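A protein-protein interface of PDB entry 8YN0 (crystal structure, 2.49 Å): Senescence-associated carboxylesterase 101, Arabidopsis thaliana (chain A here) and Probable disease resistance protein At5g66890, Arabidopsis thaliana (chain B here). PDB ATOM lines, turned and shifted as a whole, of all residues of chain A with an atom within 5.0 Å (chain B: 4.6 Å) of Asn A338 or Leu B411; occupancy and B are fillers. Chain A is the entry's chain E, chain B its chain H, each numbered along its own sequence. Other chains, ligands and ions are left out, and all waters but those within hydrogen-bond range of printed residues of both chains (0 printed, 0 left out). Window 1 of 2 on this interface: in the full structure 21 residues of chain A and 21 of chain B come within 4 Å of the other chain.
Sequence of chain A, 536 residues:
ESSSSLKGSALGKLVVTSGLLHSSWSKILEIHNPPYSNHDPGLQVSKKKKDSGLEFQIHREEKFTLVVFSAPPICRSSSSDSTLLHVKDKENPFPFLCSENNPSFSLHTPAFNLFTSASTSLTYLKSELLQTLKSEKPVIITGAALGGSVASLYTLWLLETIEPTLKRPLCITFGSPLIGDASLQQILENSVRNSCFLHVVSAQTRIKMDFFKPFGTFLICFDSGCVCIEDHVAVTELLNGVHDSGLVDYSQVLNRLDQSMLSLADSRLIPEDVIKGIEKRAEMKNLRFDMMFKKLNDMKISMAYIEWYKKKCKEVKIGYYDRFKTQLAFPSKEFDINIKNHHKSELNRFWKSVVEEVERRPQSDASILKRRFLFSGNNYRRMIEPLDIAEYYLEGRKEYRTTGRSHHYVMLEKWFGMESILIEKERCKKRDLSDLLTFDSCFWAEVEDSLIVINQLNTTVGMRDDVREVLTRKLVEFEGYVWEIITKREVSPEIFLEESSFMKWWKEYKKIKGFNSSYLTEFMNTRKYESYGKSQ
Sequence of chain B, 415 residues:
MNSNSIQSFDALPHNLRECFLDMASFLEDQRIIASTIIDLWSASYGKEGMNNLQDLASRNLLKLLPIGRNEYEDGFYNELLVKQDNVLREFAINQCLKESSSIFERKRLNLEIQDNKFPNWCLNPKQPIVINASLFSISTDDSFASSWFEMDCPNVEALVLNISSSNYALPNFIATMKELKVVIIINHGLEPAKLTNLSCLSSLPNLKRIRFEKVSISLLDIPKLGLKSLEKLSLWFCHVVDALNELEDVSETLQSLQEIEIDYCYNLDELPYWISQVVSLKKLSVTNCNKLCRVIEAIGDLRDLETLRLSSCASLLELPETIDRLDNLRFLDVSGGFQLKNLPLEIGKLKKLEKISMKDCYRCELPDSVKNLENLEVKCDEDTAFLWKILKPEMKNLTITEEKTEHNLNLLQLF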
ATOM      1  N   GLU A 334      -5.659 -26.779  17.640  1.00  0.00           N
ATOM      2  CA  GLU A 334      -6.458 -25.998  18.593  1.00  0.00           C
ATOM      3  C   GLU A 334      -7.931 -25.947  18.214  1.00  0.00           C
ATOM      4  O   GLU A 334      -8.808 -25.932  19.091  1.00  0.00           O
ATOM      5  CB  GLU A 334      -5.904 -24.572  18.701  1.00  0.00           C
ATOM      6  CG  GLU A 334      -4.526 -24.517  19.304  1.00  0.00           C
ATOM      7  CD  GLU A 334      -3.406 -24.608  18.265  1.00  0.00           C
ATOM      8  OE1 GLU A 334      -3.628 -25.052  17.113  1.00  0.00           O
ATOM      9  OE2 GLU A 334      -2.283 -24.215  18.623  1.00  0.00           O
ATOM     10  N   PHE A 335      -8.233 -25.866  16.922  1.00  0.00           N
ATOM     11  CA  PHE A 335      -9.635 -25.797  16.534  1.00  0.00           C
ATOM     12  C   PHE A 335     -10.423 -26.950  17.138  1.00  0.00           C
ATOM     13  O   PHE A 335     -11.518 -26.746  17.673  1.00  0.00           O
ATOM     14  CB  PHE A 335      -9.800 -25.798  15.021  1.00  0.00           C
ATOM     15  CG  PHE A 335     -11.177 -25.429  14.606  1.00  0.00           C
ATOM     16  CD1 PHE A 335     -11.641 -24.126  14.793  1.00  0.00           C
ATOM     17  CD2 PHE A 335     -12.041 -26.382  14.100  1.00  0.00           C
ATOM     18  CE1 PHE A 335     -12.936 -23.776  14.447  1.00  0.00           C
ATOM     19  CE2 PHE A 335     -13.341 -26.047  13.741  1.00  0.00           C
ATOM     20  CZ  PHE A 335     -13.802 -24.751  13.912  1.00  0.00           C
ATOM     21  N   ASP A 336      -9.876 -28.167  17.064  1.00  0.00           N
ATOM     22  CA  ASP A 336     -10.603 -29.338  17.533  1.00  0.00           C
ATOM     23  C   ASP A 336     -10.868 -29.248  19.025  1.00  0.00           C
ATOM     24  O   ASP A 336     -11.933 -29.665  19.510  1.00  0.00           O
ATOM     25  CB  ASP A 336      -9.811 -30.609  17.220  1.00  0.00           C
ATOM     26  CG  ASP A 336      -9.535 -30.773  15.748  1.00  0.00           C
ATOM     27  OD1 ASP A 336      -8.755 -29.992  15.200  1.00  0.00           O
ATOM     28  OD2 ASP A 336     -10.111 -31.676  15.127  1.00  0.00           O
ATOM     29  N   ILE A 337      -9.892 -28.738  19.777  1.00  0.00           N
ATOM     30  CA  ILE A 337     -10.071 -28.622  21.212  1.00  0.00           C
ATOM     31  C   ILE A 337     -11.192 -27.660  21.507  1.00  0.00           C
ATOM     32  O   ILE A 337     -11.956 -27.863  22.462  1.00  0.00           O
ATOM     33  CB  ILE A 337      -8.759 -28.199  21.879  1.00  0.00           C
ATOM     34  CG1 ILE A 337      -7.899 -29.447  22.094  1.00  0.00           C
ATOM     35  CG2 ILE A 337      -9.038 -27.428  23.177  1.00  0.00           C
ATOM     36  CD1 ILE A 337      -6.514 -29.147  22.475  1.00  0.00           C
ATOM     37  N   ASN A 338     -11.357 -26.633  20.669  1.00  0.00           N
ATOM     38  CA  ASN A 338     -12.489 -25.741  20.877  1.00  0.00           C
ATOM     39  C   ASN A 338     -13.802 -26.404  20.495  1.00  0.00           C
ATOM     40  O   ASN A 338     -14.825 -26.205  21.168  1.00  0.00           O
ATOM     41  CB  ASN A 338     -12.270 -24.457  20.103  1.00  0.00           C
ATOM     42  CG  ASN A 338     -11.502 -23.468  20.906  1.00  0.00           C
ATOM     43  OD1 ASN A 338     -12.077 -22.607  21.567  1.00  0.00           O
ATOM     44  ND2 ASN A 338     -10.178 -23.669  20.968  1.00  0.00           N
ATOM     45  N   ILE A 339     -13.798 -27.181  19.407  1.00  0.00           N
ATOM     46  CA  ILE A 339     -15.013 -27.860  18.995  1.00  0.00           C
ATOM     47  C   ILE A 339     -15.498 -28.735  20.130  1.00  0.00           C
ATOM     48  O   ILE A 339     -16.692 -28.733  20.480  1.00  0.00           O
ATOM     49  CB  ILE A 339     -14.790 -28.685  17.713  1.00  0.00           C
ATOM     50  CG1 ILE A 339     -14.778 -27.772  16.488  1.00  0.00           C
ATOM     51  CG2 ILE A 339     -15.892 -29.785  17.591  1.00  0.00           C
ATOM     52  CD1 ILE A 339     -16.048 -26.987  16.312  1.00  0.00           C
ATOM     53  N   LYS A 340     -14.570 -29.465  20.755  1.00  0.00           N
ATOM     54  CA  LYS A 340     -14.987 -30.404  21.789  1.00  0.00           C
ATOM     55  C   LYS A 340     -15.337 -29.678  23.084  1.00  0.00           C
ATOM     56  O   LYS A 340     -16.436 -29.837  23.615  1.00  0.00           O
ATOM     57  CB  LYS A 340     -13.910 -31.467  22.028  1.00  0.00           C
ATOM     58  CG  LYS A 340     -14.426 -32.607  22.867  1.00  0.00           C
ATOM     59  CD  LYS A 340     -13.392 -33.161  23.812  1.00  0.00           C
ATOM     60  CE  LYS A 340     -13.949 -34.264  24.722  1.00  0.00           C
ATOM     61  NZ  LYS A 340     -15.032 -33.801  25.667  1.00  0.00           N
ATOM     62  N   ASN A 341     -14.447 -28.834  23.582  1.00  0.00           N
ATOM     63  CA  ASN A 341     -14.655 -28.285  24.918  1.00  0.00           C
ATOM     64  C   ASN A 341     -15.523 -27.025  24.963  1.00  0.00           C
ATOM     65  O   ASN A 341     -16.096 -26.735  26.019  1.00  0.00           O
ATOM     66  CB  ASN A 341     -13.306 -27.997  25.552  1.00  0.00           C
ATOM     67  CG  ASN A 341     -12.494 -29.224  25.686  1.00  0.00           C
ATOM     68  OD1 ASN A 341     -12.580 -29.921  26.683  1.00  0.00           O
ATOM     69  ND2 ASN A 341     -11.732 -29.536  24.661  1.00  0.00           N
ATOM     70  N   HIS A 342     -15.604 -26.253  23.886  1.00  0.00           N
ATOM     71  CA  HIS A 342     -16.566 -25.147  23.844  1.00  0.00           C
ATOM     72  C   HIS A 342     -17.906 -25.723  23.405  1.00  0.00           C
ATOM     73  O   HIS A 342     -18.853 -25.823  24.186  1.00  0.00           O
ATOM     74  CB  HIS A 342     -16.248 -24.103  22.780  1.00  0.00           C
ATOM     75  CG  HIS A 342     -17.061 -22.867  22.945  1.00  0.00           C
ATOM     76  ND1 HIS A 342     -18.444 -22.891  22.945  1.00  0.00           N
ATOM     77  CD2 HIS A 342     -16.720 -21.569  22.771  1.00  0.00           C
ATOM     78  CE1 HIS A 342     -18.900 -21.653  23.012  1.00  0.00           C
ATOM     79  NE2 HIS A 342     -17.876 -20.831  22.865  1.00  0.00           N
ATOM     80  N   HIS A 343     -17.999 -26.054  22.103  1.00  0.00           N
ATOM     81  CA  HIS A 343     -19.285 -26.156  21.428  1.00  0.00           C
ATOM     82  C   HIS A 343     -19.983 -27.467  21.743  1.00  0.00           C
ATOM     83  O   HIS A 343     -21.160 -27.456  22.086  1.00  0.00           O
ATOM     84  CB  HIS A 343     -19.108 -25.998  19.919  1.00  0.00           C
ATOM     85  CG  HIS A 343     -18.638 -24.633  19.512  1.00  0.00           C
ATOM     86  ND1 HIS A 343     -19.417 -23.501  19.659  1.00  0.00           N
ATOM     87  CD2 HIS A 343     -17.468 -24.218  18.972  1.00  0.00           C
ATOM     88  CE1 HIS A 343     -18.741 -22.449  19.230  1.00  0.00           C
ATOM     89  NE2 HIS A 343     -17.554 -22.857  18.814  1.00  0.00           N
ATOM     90  N   ILE B  67      -8.542 -14.384  16.904  1.00  0.00           N
ATOM     91  CA  ILE B  67      -9.141 -15.678  17.212  1.00  0.00           C
ATOM     92  C   ILE B  67      -9.738 -15.618  18.611  1.00  0.00           C
ATOM     93  O   ILE B  67      -9.681 -16.599  19.361  1.00  0.00           O
ATOM     94  CB  ILE B  67      -8.110 -16.818  17.138  1.00  0.00           C
ATOM     95  CG1 ILE B  67      -6.995 -16.549  18.152  1.00  0.00           C
ATOM     96  CG2 ILE B  67      -7.561 -16.966  15.735  1.00  0.00           C
ATOM     97  CD1 ILE B  67      -6.027 -17.638  18.285  1.00  0.00           C
ATOM     98  N   TYR B 264      -3.488 -24.219  26.359  1.00  0.00           N
ATOM     99  CA  TYR B 264      -3.749 -25.399  25.566  1.00  0.00           C
ATOM    100  C   TYR B 264      -2.915 -26.578  26.038  1.00  0.00           C
ATOM    101  O   TYR B 264      -2.513 -27.429  25.236  1.00  0.00           O
ATOM    102  CB  TYR B 264      -3.488 -25.117  24.095  1.00  0.00           C
ATOM    103  CG  TYR B 264      -4.602 -24.381  23.448  1.00  0.00           C
ATOM    104  CD1 TYR B 264      -5.796 -25.033  23.122  1.00  0.00           C
ATOM    105  CD2 TYR B 264      -4.480 -23.033  23.150  1.00  0.00           C
ATOM    106  CE1 TYR B 264      -6.841 -24.343  22.506  1.00  0.00           C
ATOM    107  CE2 TYR B 264      -5.494 -22.351  22.555  1.00  0.00           C
ATOM    108  CZ  TYR B 264      -6.671 -23.000  22.239  1.00  0.00           C
ATOM    109  OH  TYR B 264      -7.666 -22.274  21.639  1.00  0.00           O
ATOM    110  N   ASN B 288      -7.372 -22.437  28.353  1.00  0.00           N
ATOM    111  CA  ASN B 288      -7.650 -23.583  27.494  1.00  0.00           C
ATOM    112  C   ASN B 288      -6.943 -24.829  28.002  1.00  0.00           C
ATOM    113  O   ASN B 288      -6.424 -25.628  27.226  1.00  0.00           O
ATOM    114  CB  ASN B 288      -7.261 -23.298  26.041  1.00  0.00           C
ATOM    115  CG  ASN B 288      -8.217 -22.313  25.356  1.00  0.00           C
ATOM    116  OD1 ASN B 288      -7.840 -21.182  25.048  1.00  0.00           O
ATOM    117  ND2 ASN B 288      -9.436 -22.743  25.104  1.00  0.00           N
ATOM    118  N   LEU B 409     -14.279 -17.305  11.048  1.00  0.00           N
ATOM    119  CA  LEU B 409     -13.715 -18.635  10.867  1.00  0.00           C
ATOM    120  C   LEU B 409     -12.204 -18.719  11.118  1.00  0.00           C
ATOM    121  O   LEU B 409     -11.588 -19.658  10.720  1.00  0.00           O
ATOM    122  CB  LEU B 409     -14.150 -19.203   9.531  1.00  0.00           C
ATOM    123  CG  LEU B 409     -15.621 -19.598   9.463  1.00  0.00           C
ATOM    124  CD1 LEU B 409     -15.941 -20.184   8.106  1.00  0.00           C
ATOM    125  CD2 LEU B 409     -15.994 -20.571  10.563  1.00  0.00           C
ATOM    126  N   ASN B 410     -11.627 -17.750  11.793  1.00  0.00           N
ATOM    127  CA  ASN B 410     -10.192 -17.656  11.997  1.00  0.00           C
ATOM    128  C   ASN B 410      -9.518 -18.816  12.751  1.00  0.00           C
ATOM    129  O   ASN B 410      -8.403 -19.143  12.449  1.00  0.00           O
ATOM    130  CB  ASN B 410      -9.869 -16.306  12.615  1.00  0.00           C
ATOM    131  CG  ASN B 410     -10.124 -15.141  11.680  1.00  0.00           C
ATOM    132  OD1 ASN B 410     -10.374 -15.314  10.501  1.00  0.00           O
ATOM    133  ND2 ASN B 410     -10.060 -13.940  12.218  1.00  0.00           N
ATOM    134  N   LEU B 411     -10.163 -19.406  13.732  1.00  0.00           N
ATOM    135  CA  LEU B 411      -9.625 -20.551  14.484  1.00  0.00           C
ATOM    136  C   LEU B 411      -9.442 -21.743  13.558  1.00  0.00           C
ATOM    137  O   LEU B 411      -8.685 -22.627  13.856  1.00  0.00           O
ATOM    138  CB  LEU B 411     -10.439 -20.852  15.730  1.00  0.00           C
ATOM    139  CG  LEU B 411      -9.781 -21.579  16.882  1.00  0.00           C
ATOM    140  CD1 LEU B 411      -8.594 -20.778  17.362  1.00  0.00           C
ATOM    141  CD2 LEU B 411     -10.807 -21.716  17.980  1.00  0.00           C
ATOM    142  N   LEU B 412     -10.138 -21.764  12.451  1.00  0.00           N
ATOM    143  CA  LEU B 412      -9.993 -22.813  11.454  1.00  0.00           C
ATOM    144  C   LEU B 412      -8.586 -22.807  10.887  1.00  0.00           C
ATOM    145  O   LEU B 412      -8.153 -23.785  10.331  1.00  0.00           O
ATOM    146  CB  LEU B 412     -11.059 -22.738  10.376  1.00  0.00           C
ATOM    147  CG  LEU B 412     -12.242 -23.668  10.544  1.00  0.00           C
ATOM    148  CD1 LEU B 412     -13.278 -23.353   9.487  1.00  0.00           C
ATOM    149  CD2 LEU B 412     -11.780 -25.108  10.447  1.00  0.00           C
ATOM    150  N   GLN B 413      -7.892 -21.702  10.947  1.00  0.00           N
ATOM    151  CA  GLN B 413      -6.508 -21.681  10.545  1.00  0.00           C
ATOM    152  C   GLN B 413      -5.734 -22.635  11.434  1.00  0.00           C
ATOM    153  O   GLN B 413      -4.767 -23.214  11.005  1.00  0.00           O
ATOM    154  CB  GLN B 413      -5.965 -20.286  10.635  1.00  0.00           C
ATOM    155  CG  GLN B 413      -6.576 -19.297   9.674  1.00  0.00           C
ATOM    156  CD  GLN B 413      -5.954 -19.379   8.310  1.00  0.00           C
ATOM    157  OE1 GLN B 413      -4.841 -19.851   8.155  1.00  0.00           O
ATOM    158  NE2 GLN B 413      -6.668 -18.908   7.314  1.00  0.00           N
ATOM    159  N   LEU B 414      -6.074 -22.707  12.698  1.00  0.00           N
ATOM    160  CA  LEU B 414      -5.466 -23.668  13.613  1.00  0.00           C
ATOM    161  C   LEU B 414      -6.129 -25.038  13.506  1.00  0.00           C
ATOM    162  O   LEU B 414      -6.501 -25.609  14.496  1.00  0.00           O
ATOM    163  CB  LEU B 414      -5.474 -23.100  15.026  1.00  0.00           C
ATOM    164  CG  LEU B 414      -4.869 -21.721  15.205  1.00  0.00           C
ATOM    165  CD1 LEU B 414      -4.936 -21.323  16.662  1.00  0.00           C
ATOM    166  CD2 LEU B 414      -3.437 -21.734  14.725  1.00  0.00           C
ATOM    167  N   PHE B 415      -6.268 -25.555  12.301  1.00  0.00           N
ATOM    168  CA  PHE B 415      -6.845 -26.850  11.994  1.00  0.00           C
ATOM    169  C   PHE B 415      -5.854 -27.607  11.131  1.00  0.00           C
ATOM    170  O   PHE B 415      -5.533 -28.784  11.353  1.00  0.00           O
ATOM    171  CB  PHE B 415      -8.174 -26.688  11.257  1.00  0.00           C
ATOM    172  CG  PHE B 415      -8.763 -27.985  10.779  1.00  0.00           C
ATOM    173  CD1 PHE B 415      -8.298 -28.599   9.626  1.00  0.00           C
ATOM    174  CD2 PHE B 415      -9.798 -28.592  11.481  1.00  0.00           C
ATOM    175  CE1 PHE B 415      -8.848 -29.806   9.187  1.00  0.00           C
ATOM    176  CE2 PHE B 415     -10.349 -29.797  11.040  1.00  0.00           C
ATOM    177  CZ  PHE B 415      -9.870 -30.396   9.894  1.00  0.00           C
ATOM    178  OXT PHE B 415      -5.364 -27.003  10.168  1.00  0.00           O
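Printed residues of chain B that touch a printed residue of chain A: Tyr B264, Leu B411, Leu B412 and Leu B414. Hydrophobic or aromatic side chains of chain B within 4 Å of the printed part of chain A: Tyr B264, Leu B411, Leu B412 and Leu B414. Printed residues of chain A that touch a printed residue of chain B: Glu A334, Phe A335, Ile A337 and Asn A338. Hydrophobic or aromatic side chains of chain A within 4 Å of the printed part of chain B: Phe A335 and Ile A337. Among the printed residues, no Asp or Glu carboxylate lies within 4 Å of a Lys or Arg side-chain nitrogen of the other chain.
Among the printed residues, merely in contact across the chains: Glu A334 with Tyr B264 (3.9 Å), Phe A335 with Leu B411 (3.4 Å), Phe A335 with Leu B412 (3.7 Å), Ile A337 with Tyr B264 (3.8 Å) and Asn A338 with Leu B411 (3.5 Å).
Of the printed residues of chain B, Phe A335 touches Leu B411 (3.4 Å), Leu B412 (3.7 Å) and Leu B414 (3.0 Å). Printed residues of chain B within 4 Å of Ile A337: Tyr B264. Of chain B, only Tyr B264 and Leu B411 come within 4 Å of Asn A338. Asn A341 touches none of the printed residues of chain B. His A342 touches none of the printed residues of chain B. Printed residues of chain A within 4 Å of Leu B414: Glu A334 (3.4 Å) and Phe A335 (3.0 Å). The nearest printed residue of chain B that does not touch Ile A337 is Asn B288 (5.1 Å).
The backbone carbonyl oxygen (O) of Leu B414 lies within hydrogen-bond range of the backbone NH (N) of Glu A334, at 3.5 Å. The backbone NH of Phe A335 lies within hydrogen-bond range of the backbone carbonyl oxygen of Leu B414, at 3.0 Å. ND2 of Asn A338 sits at hydrogen-bond distance from OH of Tyr B264, at 3.0 Å.
O of Glu A334 lies within hydrogen-bond range of ND2 of Asn A338 (3.2 Å). The side-chain amide nitrogen (ND2) of Asn A341 is in hydrogen-bond range of the backbone carbonyl oxygen (O) of Ile A337, 2.8 Å away. The backbone carbonyl oxygen (O) of Asn A338 sits at hydrogen-bond distance from the backbone NH (N) of His A343, at 3.3 Å. N of Tyr B264 sits close to O of Asn B288 (3.4 Å).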
